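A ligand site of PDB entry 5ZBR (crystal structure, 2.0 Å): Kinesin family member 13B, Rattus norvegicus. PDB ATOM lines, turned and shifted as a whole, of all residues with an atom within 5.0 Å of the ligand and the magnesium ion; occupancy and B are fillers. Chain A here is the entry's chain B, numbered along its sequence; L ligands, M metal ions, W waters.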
ATOM      1  N   ARG A   9     -12.241  15.490  17.102  1.00  0.00           N
ATOM      2  CA  ARG A   9     -11.413  15.534  18.294  1.00  0.00           C
ATOM      3  C   ARG A   9     -10.727  16.891  18.368  1.00  0.00           C
ATOM      4  O   ARG A   9      -9.921  17.216  17.496  1.00  0.00           O
ATOM      5  CB  ARG A   9     -10.375  14.422  18.294  1.00  0.00           C
ATOM      6  CG  ARG A   9      -9.649  14.328  19.639  1.00  0.00           C
ATOM      7  CD  ARG A   9      -8.620  13.190  19.719  1.00  0.00           C
ATOM      8  NE  ARG A   9      -8.238  12.902  21.105  1.00  0.00           N
ATOM      9  CZ  ARG A   9      -7.329  12.018  21.485  1.00  0.00           C
ATOM     10  NH1 ARG A   9      -6.654  11.341  20.567  1.00  0.00           N
ATOM     11  NH2 ARG A   9      -7.066  11.792  22.772  1.00  0.00           N
ATOM     12  N   VAL A  10     -11.049  17.652  19.406  1.00  0.00           N
ATOM     13  CA  VAL A  10     -10.407  18.942  19.693  1.00  0.00           C
ATOM     14  C   VAL A  10      -9.233  18.691  20.613  1.00  0.00           C
ATOM     15  O   VAL A  10      -9.407  18.165  21.716  1.00  0.00           O
ATOM     16  CB  VAL A  10     -11.384  19.935  20.334  1.00  0.00           C
ATOM     17  CG1 VAL A  10     -10.735  21.335  20.395  1.00  0.00           C
ATOM     18  CG2 VAL A  10     -12.724  19.953  19.566  1.00  0.00           C
ATOM     19  N   ARG A  11      -8.036  19.064  20.175  1.00  0.00           N
ATOM     20  CA  ARG A  11      -6.891  18.934  21.041  1.00  0.00           C
ATOM     21  C   ARG A  11      -6.862  20.131  21.982  1.00  0.00           C
ATOM     22  O   ARG A  11      -7.420  21.196  21.694  1.00  0.00           O
ATOM     23  CB  ARG A  11      -5.607  18.844  20.239  1.00  0.00           C
ATOM     24  CG  ARG A  11      -5.210  20.114  19.536  1.00  0.00           C
ATOM     25  CD  ARG A  11      -3.639  20.281  19.492  1.00  0.00           C
ATOM     26  NE  ARG A  11      -3.306  21.438  18.685  1.00  0.00           N
ATOM     27  CZ  ARG A  11      -3.198  22.681  19.157  1.00  0.00           C
ATOM     28  NH1 ARG A  11      -3.356  22.949  20.450  1.00  0.00           N
ATOM     29  NH2 ARG A  11      -2.901  23.678  18.339  1.00  0.00           N
ATOM     30  N   PRO A  12      -6.231  19.972  23.139  1.00  0.00           N
ATOM     31  CA  PRO A  12      -6.221  21.054  24.116  1.00  0.00           C
ATOM     32  C   PRO A  12      -5.320  22.174  23.653  1.00  0.00           C
ATOM     33  O   PRO A  12      -4.456  22.008  22.779  1.00  0.00           O
ATOM     34  CB  PRO A  12      -5.673  20.399  25.388  1.00  0.00           C
ATOM     35  CG  PRO A  12      -4.931  19.185  24.887  1.00  0.00           C
ATOM     36  CD  PRO A  12      -5.710  18.709  23.719  1.00  0.00           C
ATOM     37  N   SER A  62     -10.680  17.789  25.522  1.00  0.00           N
ATOM     38  CA  SER A  62      -9.795  17.678  26.686  1.00  0.00           C
ATOM     39  C   SER A  62      -9.728  18.980  27.486  1.00  0.00           C
ATOM     40  O   SER A  62      -9.553  20.060  26.920  1.00  0.00           O
ATOM     41  CB  SER A  62      -8.383  17.276  26.270  1.00  0.00           C
ATOM     42  OG  SER A  62      -8.396  16.049  25.559  1.00  0.00           O
ATOM     43  N   GLU A  65      -3.736  19.544  29.182  1.00  0.00           N
ATOM     44  CA  GLU A  65      -2.789  18.501  28.812  1.00  0.00           C
ATOM     45  C   GLU A  65      -2.157  17.824  30.034  1.00  0.00           C
ATOM     46  O   GLU A  65      -1.054  17.286  29.935  1.00  0.00           O
ATOM     47  CB  GLU A  65      -1.698  19.050  27.903  1.00  0.00           C
ATOM     48  CG  GLU A  65      -2.112  20.203  27.017  1.00  0.00           C
ATOM     49  CD  GLU A  65      -0.960  20.732  26.190  1.00  0.00           C
ATOM     50  OE1 GLU A  65      -0.650  20.124  25.141  1.00  0.00           O
ATOM     51  OE2 GLU A  65      -0.343  21.750  26.603  1.00  0.00           O
ATOM     52  N   LYS A  70      -4.746  13.293  29.498  1.00  0.00           N
ATOM     53  CA  LYS A  70      -4.241  12.559  28.348  1.00  0.00           C
ATOM     54  C   LYS A  70      -4.635  11.082  28.425  1.00  0.00           C
ATOM     55  O   LYS A  70      -5.094  10.504  27.425  1.00  0.00           O
ATOM     56  CB  LYS A  70      -2.726  12.719  28.259  1.00  0.00           C
ATOM     57  CG  LYS A  70      -2.283  14.133  27.868  1.00  0.00           C
ATOM     58  CD  LYS A  70      -0.877  14.120  27.285  1.00  0.00           C
ATOM     59  CE  LYS A  70       0.129  14.611  28.305  1.00  0.00           C
ATOM     60  NZ  LYS A  70       1.148  15.474  27.645  1.00  0.00           N
ATOM     61  N   GLY A 101      -7.080  16.337   9.237  1.00  0.00           N
ATOM     62  CA  GLY A 101      -7.073  17.658   9.842  1.00  0.00           C
ATOM     63  C   GLY A 101      -5.740  18.353   9.598  1.00  0.00           C
ATOM     64  O   GLY A 101      -4.803  17.783   9.028  1.00  0.00           O
ATOM     65  N   GLN A 102      -5.689  19.607  10.037  1.00  0.00           N
ATOM     66  CA  GLN A 102      -4.498  20.403   9.742  1.00  0.00           C
ATOM     67  C   GLN A 102      -3.312  19.881  10.532  1.00  0.00           C
ATOM     68  O   GLN A 102      -3.453  19.147  11.520  1.00  0.00           O
ATOM     69  CB  GLN A 102      -4.733  21.888  10.029  1.00  0.00           C
ATOM     70  CG  GLN A 102      -4.455  22.307  11.458  1.00  0.00           C
ATOM     71  CD  GLN A 102      -4.644  23.790  11.682  1.00  0.00           C
ATOM     72  OE1 GLN A 102      -5.569  24.199  12.358  1.00  0.00           O
ATOM     73  NE2 GLN A 102      -3.749  24.597  11.133  1.00  0.00           N
ATOM     74  N   THR A 103      -2.122  20.236  10.057  1.00  0.00           N
ATOM     75  CA  THR A 103      -0.904  19.888  10.794  1.00  0.00           C
ATOM     76  C   THR A 103      -0.948  20.482  12.198  1.00  0.00           C
ATOM     77  O   THR A 103      -1.400  21.614  12.391  1.00  0.00           O
ATOM     78  CB  THR A 103       0.341  20.404  10.049  1.00  0.00           C
ATOM     79  OG1 THR A 103       0.499  19.662   8.842  1.00  0.00           O
ATOM     80  CG2 THR A 103       1.596  20.233  10.899  1.00  0.00           C
ATOM     81  N   GLY A 104      -0.496  19.695  13.170  1.00  0.00           N
ATOM     82  CA  GLY A 104      -0.540  20.048  14.563  1.00  0.00           C
ATOM     83  C   GLY A 104      -1.841  19.757  15.278  1.00  0.00           C
ATOM     84  O   GLY A 104      -1.906  19.949  16.505  1.00  0.00           O
ATOM     85  N   SER A 105      -2.889  19.293  14.590  1.00  0.00           N
ATOM     86  CA  SER A 105      -4.178  19.168  15.254  1.00  0.00           C
ATOM     87  C   SER A 105      -4.380  17.835  15.983  1.00  0.00           C
ATOM     88  O   SER A 105      -5.319  17.730  16.776  1.00  0.00           O
ATOM     89  CB  SER A 105      -5.349  19.396  14.290  1.00  0.00           C
ATOM     90  OG  SER A 105      -5.373  18.471  13.220  1.00  0.00           O
ATOM     91  N   GLY A 106      -3.544  16.828  15.732  1.00  0.00           N
ATOM     92  CA  GLY A 106      -3.588  15.623  16.542  1.00  0.00           C
ATOM     93  C   GLY A 106      -3.842  14.322  15.795  1.00  0.00           C
ATOM     94  O   GLY A 106      -4.249  13.311  16.409  1.00  0.00           O
ATOM     95  N   LYS A 107      -3.599  14.328  14.480  1.00  0.00           N
ATOM     96  CA  LYS A 107      -3.835  13.119  13.698  1.00  0.00           C
ATOM     97  C   LYS A 107      -2.980  11.961  14.193  1.00  0.00           C
ATOM     98  O   LYS A 107      -3.503  10.886  14.526  1.00  0.00           O
ATOM     99  CB  LYS A 107      -3.584  13.388  12.214  1.00  0.00           C
ATOM    100  CG  LYS A 107      -4.615  14.297  11.552  1.00  0.00           C
ATOM    101  CD  LYS A 107      -4.286  14.500  10.063  1.00  0.00           C
ATOM    102  CE  LYS A 107      -2.829  15.011   9.901  1.00  0.00           C
ATOM    103  NZ  LYS A 107      -2.577  16.364  10.395  1.00  0.00           N
ATOM    104  N   SER A 108      -1.657  12.144  14.223  1.00  0.00           N
ATOM    105  CA  SER A 108      -0.771  11.042  14.635  1.00  0.00           C
ATOM    106  C   SER A 108      -0.944  10.708  16.114  1.00  0.00           C
ATOM    107  O   SER A 108      -0.834   9.537  16.512  1.00  0.00           O
ATOM    108  CB  SER A 108       0.691  11.405  14.358  1.00  0.00           C
ATOM    109  OG  SER A 108       0.916  11.545  12.972  1.00  0.00           O
ATOM    110  N   TYR A 109      -1.144  11.726  16.949  1.00  0.00           N
ATOM    111  CA  TYR A 109      -1.428  11.458  18.362  1.00  0.00           C
ATOM    112  C   TYR A 109      -2.660  10.579  18.529  1.00  0.00           C
ATOM    113  O   TYR A 109      -2.739   9.739  19.452  1.00  0.00           O
ATOM    114  CB  TYR A 109      -1.604  12.792  19.093  1.00  0.00           C
ATOM    115  CG  TYR A 109      -1.879  12.632  20.564  1.00  0.00           C
ATOM    116  CD1 TYR A 109      -0.829  12.484  21.466  1.00  0.00           C
ATOM    117  CD2 TYR A 109      -3.186  12.613  21.059  1.00  0.00           C
ATOM    118  CE1 TYR A 109      -1.062  12.330  22.825  1.00  0.00           C
ATOM    119  CE2 TYR A 109      -3.442  12.447  22.433  1.00  0.00           C
ATOM    120  CZ  TYR A 109      -2.359  12.307  23.311  1.00  0.00           C
ATOM    121  OH  TYR A 109      -2.550  12.164  24.656  1.00  0.00           O
ATOM    122  N   THR A 110      -3.665  10.769  17.698  1.00  0.00           N
ATOM    123  CA  THR A 110      -4.857   9.937  17.787  1.00  0.00           C
ATOM    124  C   THR A 110      -4.605   8.529  17.259  1.00  0.00           C
ATOM    125  O   THR A 110      -5.088   7.552  17.838  1.00  0.00           O
ATOM    126  CB  THR A 110      -6.020  10.596  17.030  1.00  0.00           C
ATOM    127  OG1 THR A 110      -6.317  11.868  17.637  1.00  0.00           O
ATOM    128  CG2 THR A 110      -7.281   9.690  17.072  1.00  0.00           C
ATOM    129  N   ARG A 206       9.019   6.291   8.314  1.00  0.00           N
ATOM    130  CA  ARG A 206       8.129   7.257   7.679  1.00  0.00           C
ATOM    131  C   ARG A 206       8.897   8.509   7.296  1.00  0.00           C
ATOM    132  O   ARG A 206       9.726   9.007   8.073  1.00  0.00           O
ATOM    133  CB  ARG A 206       6.964   7.598   8.620  1.00  0.00           C
ATOM    134  CG  ARG A 206       5.694   7.932   7.887  1.00  0.00           C
ATOM    135  CD  ARG A 206       4.611   8.305   8.817  1.00  0.00           C
ATOM    136  NE  ARG A 206       3.594   9.106   8.167  1.00  0.00           N
ATOM    137  CZ  ARG A 206       2.484   9.514   8.784  1.00  0.00           C
ATOM    138  NH1 ARG A 206       2.312   9.191  10.065  1.00  0.00           N
ATOM    139  NH2 ARG A 206       1.563  10.235   8.149  1.00  0.00           N
ATOM    140  N   SER A 218       4.632  16.581   7.007  1.00  0.00           N
ATOM    141  CA  SER A 218       3.187  16.637   7.092  1.00  0.00           C
ATOM    142  C   SER A 218       2.525  16.384   5.762  1.00  0.00           C
ATOM    143  O   SER A 218       1.300  16.509   5.692  1.00  0.00           O
ATOM    144  CB  SER A 218       2.761  17.999   7.631  1.00  0.00           C
ATOM    145  OG  SER A 218       3.402  19.044   6.905  1.00  0.00           O
ATOM    146  N   ASP A 251      -3.407   7.592   8.710  1.00  0.00           N
ATOM    147  CA  ASP A 251      -2.960   8.835   9.310  1.00  0.00           C
ATOM    148  C   ASP A 251      -2.620   9.737   8.115  1.00  0.00           C
ATOM    149  O   ASP A 251      -1.626   9.508   7.431  1.00  0.00           O
ATOM    150  CB  ASP A 251      -1.777   8.565  10.241  1.00  0.00           C
ATOM    151  CG  ASP A 251      -1.245   9.844  10.907  1.00  0.00           C
ATOM    152  OD1 ASP A 251      -0.225   9.755  11.630  1.00  0.00           O
ATOM    153  OD2 ASP A 251      -1.855  10.909  10.739  1.00  0.00           O
ATOM    154  N   LEU A 252      -3.484  10.696   7.825  1.00  0.00           N
ATOM    155  CA  LEU A 252      -3.347  11.446   6.580  1.00  0.00           C
ATOM    156  C   LEU A 252      -2.285  12.545   6.704  1.00  0.00           C
ATOM    157  O   LEU A 252      -1.836  12.905   7.805  1.00  0.00           O
ATOM    158  CB  LEU A 252      -4.676  12.070   6.166  1.00  0.00           C
ATOM    159  CG  LEU A 252      -5.798  11.132   5.706  1.00  0.00           C
ATOM    160  CD1 LEU A 252      -7.089  11.909   5.577  1.00  0.00           C
ATOM    161  CD2 LEU A 252      -5.453  10.426   4.360  1.00  0.00           C
ATOM    162  N   ALA A 253      -1.885  13.074   5.560  1.00  0.00           N
ATOM    163  CA  ALA A 253      -1.123  14.311   5.522  1.00  0.00           C
ATOM    164  C   ALA A 253      -2.011  15.473   5.959  1.00  0.00           C
ATOM    165  O   ALA A 253      -3.237  15.446   5.833  1.00  0.00           O
ATOM    166  CB  ALA A 253      -0.589  14.558   4.116  1.00  0.00           C
ATOM    167  N   GLY A 254      -1.373  16.518   6.473  1.00  0.00           N
ATOM    168  CA  GLY A 254      -2.093  17.691   6.940  1.00  0.00           C
ATOM    169  C   GLY A 254      -2.944  18.393   5.903  1.00  0.00           C
ATOM    170  O   GLY A 254      -2.498  18.660   4.784  1.00  0.00           O
ATOM    171  N   THR A 327      -9.554  15.950  13.283  1.00  0.00           N
ATOM    172  CA  THR A 327      -8.831  16.584  14.376  1.00  0.00           C
ATOM    173  C   THR A 327      -8.781  18.084  14.125  1.00  0.00           C
ATOM    174  O   THR A 327      -8.548  18.508  12.988  1.00  0.00           O
ATOM    175  CB  THR A 327      -7.423  16.008  14.524  1.00  0.00           C
ATOM    176  OG1 THR A 327      -6.772  16.036  13.262  1.00  0.00           O
ATOM    177  CG2 THR A 327      -7.484  14.541  14.994  1.00  0.00           C
HETATM  178  P1  LIG L   1       1.031  16.509  11.086  1.00  0.00           P
HETATM  179  O1  LIG L   1       1.648  15.070  11.030  1.00  0.00           O
HETATM  180  O2  LIG L   1      -0.038  16.749   9.920  1.00  0.00           O
HETATM  181  O3  LIG L   1       2.218  17.371  10.767  1.00  0.00           O
HETATM  182  P2  LIG L   1      -0.570  15.980  13.490  1.00  0.00           P
HETATM  183  O4  LIG L   1      -0.212  14.552  13.206  1.00  0.00           O
HETATM  184  O5  LIG L   1      -2.046  16.289  13.092  1.00  0.00           O
HETATM  185  N1  LIG L   1       0.466  16.998  12.628  1.00  0.00           N
HETATM  186  P3  LIG L   1       0.112  15.424  16.176  1.00  0.00           P
HETATM  187  O6  LIG L   1      -0.765  14.193  16.360  1.00  0.00           O
HETATM  188  O7  LIG L   1       1.531  15.122  15.934  1.00  0.00           O
HETATM  189  O8  LIG L   1      -0.433  16.375  15.000  1.00  0.00           O
HETATM  190  O9  LIG L   1      -0.034  16.349  17.436  1.00  0.00           O
HETATM  191  C1  LIG L   1       0.842  17.453  17.712  1.00  0.00           C
HETATM  192  C2  LIG L   1       1.153  17.361  19.182  1.00  0.00           C
HETATM  193  O10 LIG L   1       0.057  17.926  19.934  1.00  0.00           O
HETATM  194  C3  LIG L   1       1.301  15.930  19.695  1.00  0.00           C
HETATM  195  O11 LIG L   1       2.651  15.484  19.579  1.00  0.00           O
HETATM  196  C4  LIG L   1       0.877  16.054  21.166  1.00  0.00           C
HETATM  197  O12 LIG L   1       1.960  16.482  21.988  1.00  0.00           O
HETATM  198  C5  LIG L   1      -0.175  17.157  21.102  1.00  0.00           C
HETATM  199  N2  LIG L   1      -1.549  16.663  21.047  1.00  0.00           N
HETATM  200  C6  LIG L   1      -2.302  16.424  19.928  1.00  0.00           C
HETATM  201  N3  LIG L   1      -3.513  16.006  20.185  1.00  0.00           N
HETATM  202  C7  LIG L   1      -3.565  15.938  21.570  1.00  0.00           C
HETATM  203  C8  LIG L   1      -4.576  15.569  22.471  1.00  0.00           C
HETATM  204  N4  LIG L   1      -5.792  15.173  22.085  1.00  0.00           N
HETATM  205  N5  LIG L   1      -4.312  15.666  23.796  1.00  0.00           N
HETATM  206  C9  LIG L   1      -3.096  16.071  24.177  1.00  0.00           C
HETATM  207  N6  LIG L   1      -2.058  16.444  23.422  1.00  0.00           N
HETATM  208  C10 LIG L   1      -2.363  16.358  22.112  1.00  0.00           C
HETATM  209 MG    MG M   1       1.198  13.441  11.993  1.00  0.00          MG
HETATM  210  O   HOH W   1       1.804  13.014  18.216  1.00  0.00           O
HETATM  211  O   HOH W   2       3.627  14.387  23.514  1.00  0.00           O
HETATM  212  O   HOH W   3       2.433  14.123  13.519  1.00  0.00           O
HETATM  213  O   HOH W   4      -0.086  12.849  10.699  1.00  0.00           O
HETATM  214  O   HOH W   5       2.861  12.649  10.613  1.00  0.00           O
HETATM  215  O   HOH W   6      -5.909  14.473  19.426  1.00  0.00           O
HETATM  216  O   HOH W   7      -6.050  14.804  25.696  1.00  0.00           O
HETATM  217  O   HOH W   8       2.440  20.325  17.279  1.00  0.00           O
HETATM  218  O   HOH W   9       2.739  17.632  14.011  1.00  0.00           O
HETATM  219  O   HOH W  10      -0.532  21.002  20.625  1.00  0.00           O
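O6 of the ligand is in hydrogen-bond range of N of Tyr 109 (2.6 Å).
NZ of Lys 107 lies within salt-bridge range of O2 of the ligand, 2.6 Å away.
An oxygen (O2) of the ligand sits at hydrogen-bond distance from the side-chain hydroxyl (OG1) of Thr 103.
The backbone NH (N) of Ser 108 sits at hydrogen-bond distance from an oxygen (O6) of the ligand (3.1 Å).
N of Lys 107 sits at hydrogen-bond distance from O5 of the ligand.
N of Gly 106 is in hydrogen-bond range of O5 of the ligand (3.1 Å).
The backbone NH (N) of Ser 105 sits at hydrogen-bond distance from an oxygen (O5) of the ligand (3.5 Å).
The side-chain hydroxyl (OG) of Ser 105 is in hydrogen-bond range of the side-chain hydroxyl (OG1) of Thr 327 (2.8 Å).
The backbone carbonyl oxygen (O) of Gln 102 lies within hydrogen-bond range of the side-chain hydroxyl (OG) of Ser 105 (2.7 Å).
The guanidinium group (NE) of Arg 11 is in hydrogen-bond range of the backbone carbonyl oxygen (O) of Gly 104, 3.0 Å away.
NZ of Lys 107 sits at hydrogen-bond distance from O of Gly 101 (3.0 Å).
OG of Ser 108 lies close to OD1 of Asp 251, at 2.5 Å.
NZ of Lys 107 sits at hydrogen-bond distance from O of Gln 102 (3.1 Å).
The side-chain hydroxyl of Thr 110 is in hydrogen-bond range of the backbone carbonyl oxygen of Gly 106 (2.8 Å).
The guanidinium group of Arg 9 is in hydrogen-bond range of the side-chain hydroxyl of Thr 110 (3.0 Å).
NE of Arg 9 lies close to N4 of the ligand, at 3.5 Å.
N1 of the ligand sits close to N of Gly 104 (2.9 Å).
Residues that only touch the ligand: Ser 218, Pro 12, Arg 11, Gln 102 and Gly 254.
13 residues have an atom within 4 Å of the ligand: Arg 9, Arg 11, Pro 12, Gln 102, Thr 103, Gly 104, Ser 105, Gly 106, Lys 107, Ser 108, Tyr 109, Ser 218 and Gly 254.
Residues that only touch the magnesium ion: Asp 251.
Of the 24 residues printed, 2 come within 4 Å of the magnesium ion.
The nearest printed residue that does not touch the magnesium ion is Lys 107 (4.8 Å).
The magnesium ion is bound by water W4 (1.9 Å), an oxygen (O1) of the ligand (1.9 Å), water W3 (2.1 Å), the side-chain hydroxyl of Ser 108 (2.2 Å), an oxygen (O4) of the ligand (2.2 Å) and water W5 (2.3 Å).
The magnesium ion has six donor atoms within binding distance.
Water W4 lies within hydrogen-bond range of OD2 of Asp 251 (2.6 Å) and O of Leu 252 (3.4 Å).
Water W7 lies within hydrogen-bond range of the side-chain hydroxyl (OG) of Ser 62 (2.7 Å) and a nitrogen (N5) of the ligand (2.7 Å).
Water W6 lies within hydrogen-bond range of a nitrogen (N4) of the ligand (2.8 Å), the side-chain hydroxyl (OG1) of Thr 110 (3.2 Å) and the guanidinium group (NE) of Arg 9 (3.3 Å).
Water W1 bridges an oxygen (O11) of the ligand (2.9 Å) and the backbone NH of Tyr 109 (3.5 Å).
Water W10 lies within hydrogen-bond range of O10 of the ligand (3.2 Å) and NE of Arg 11 (3.4 Å).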
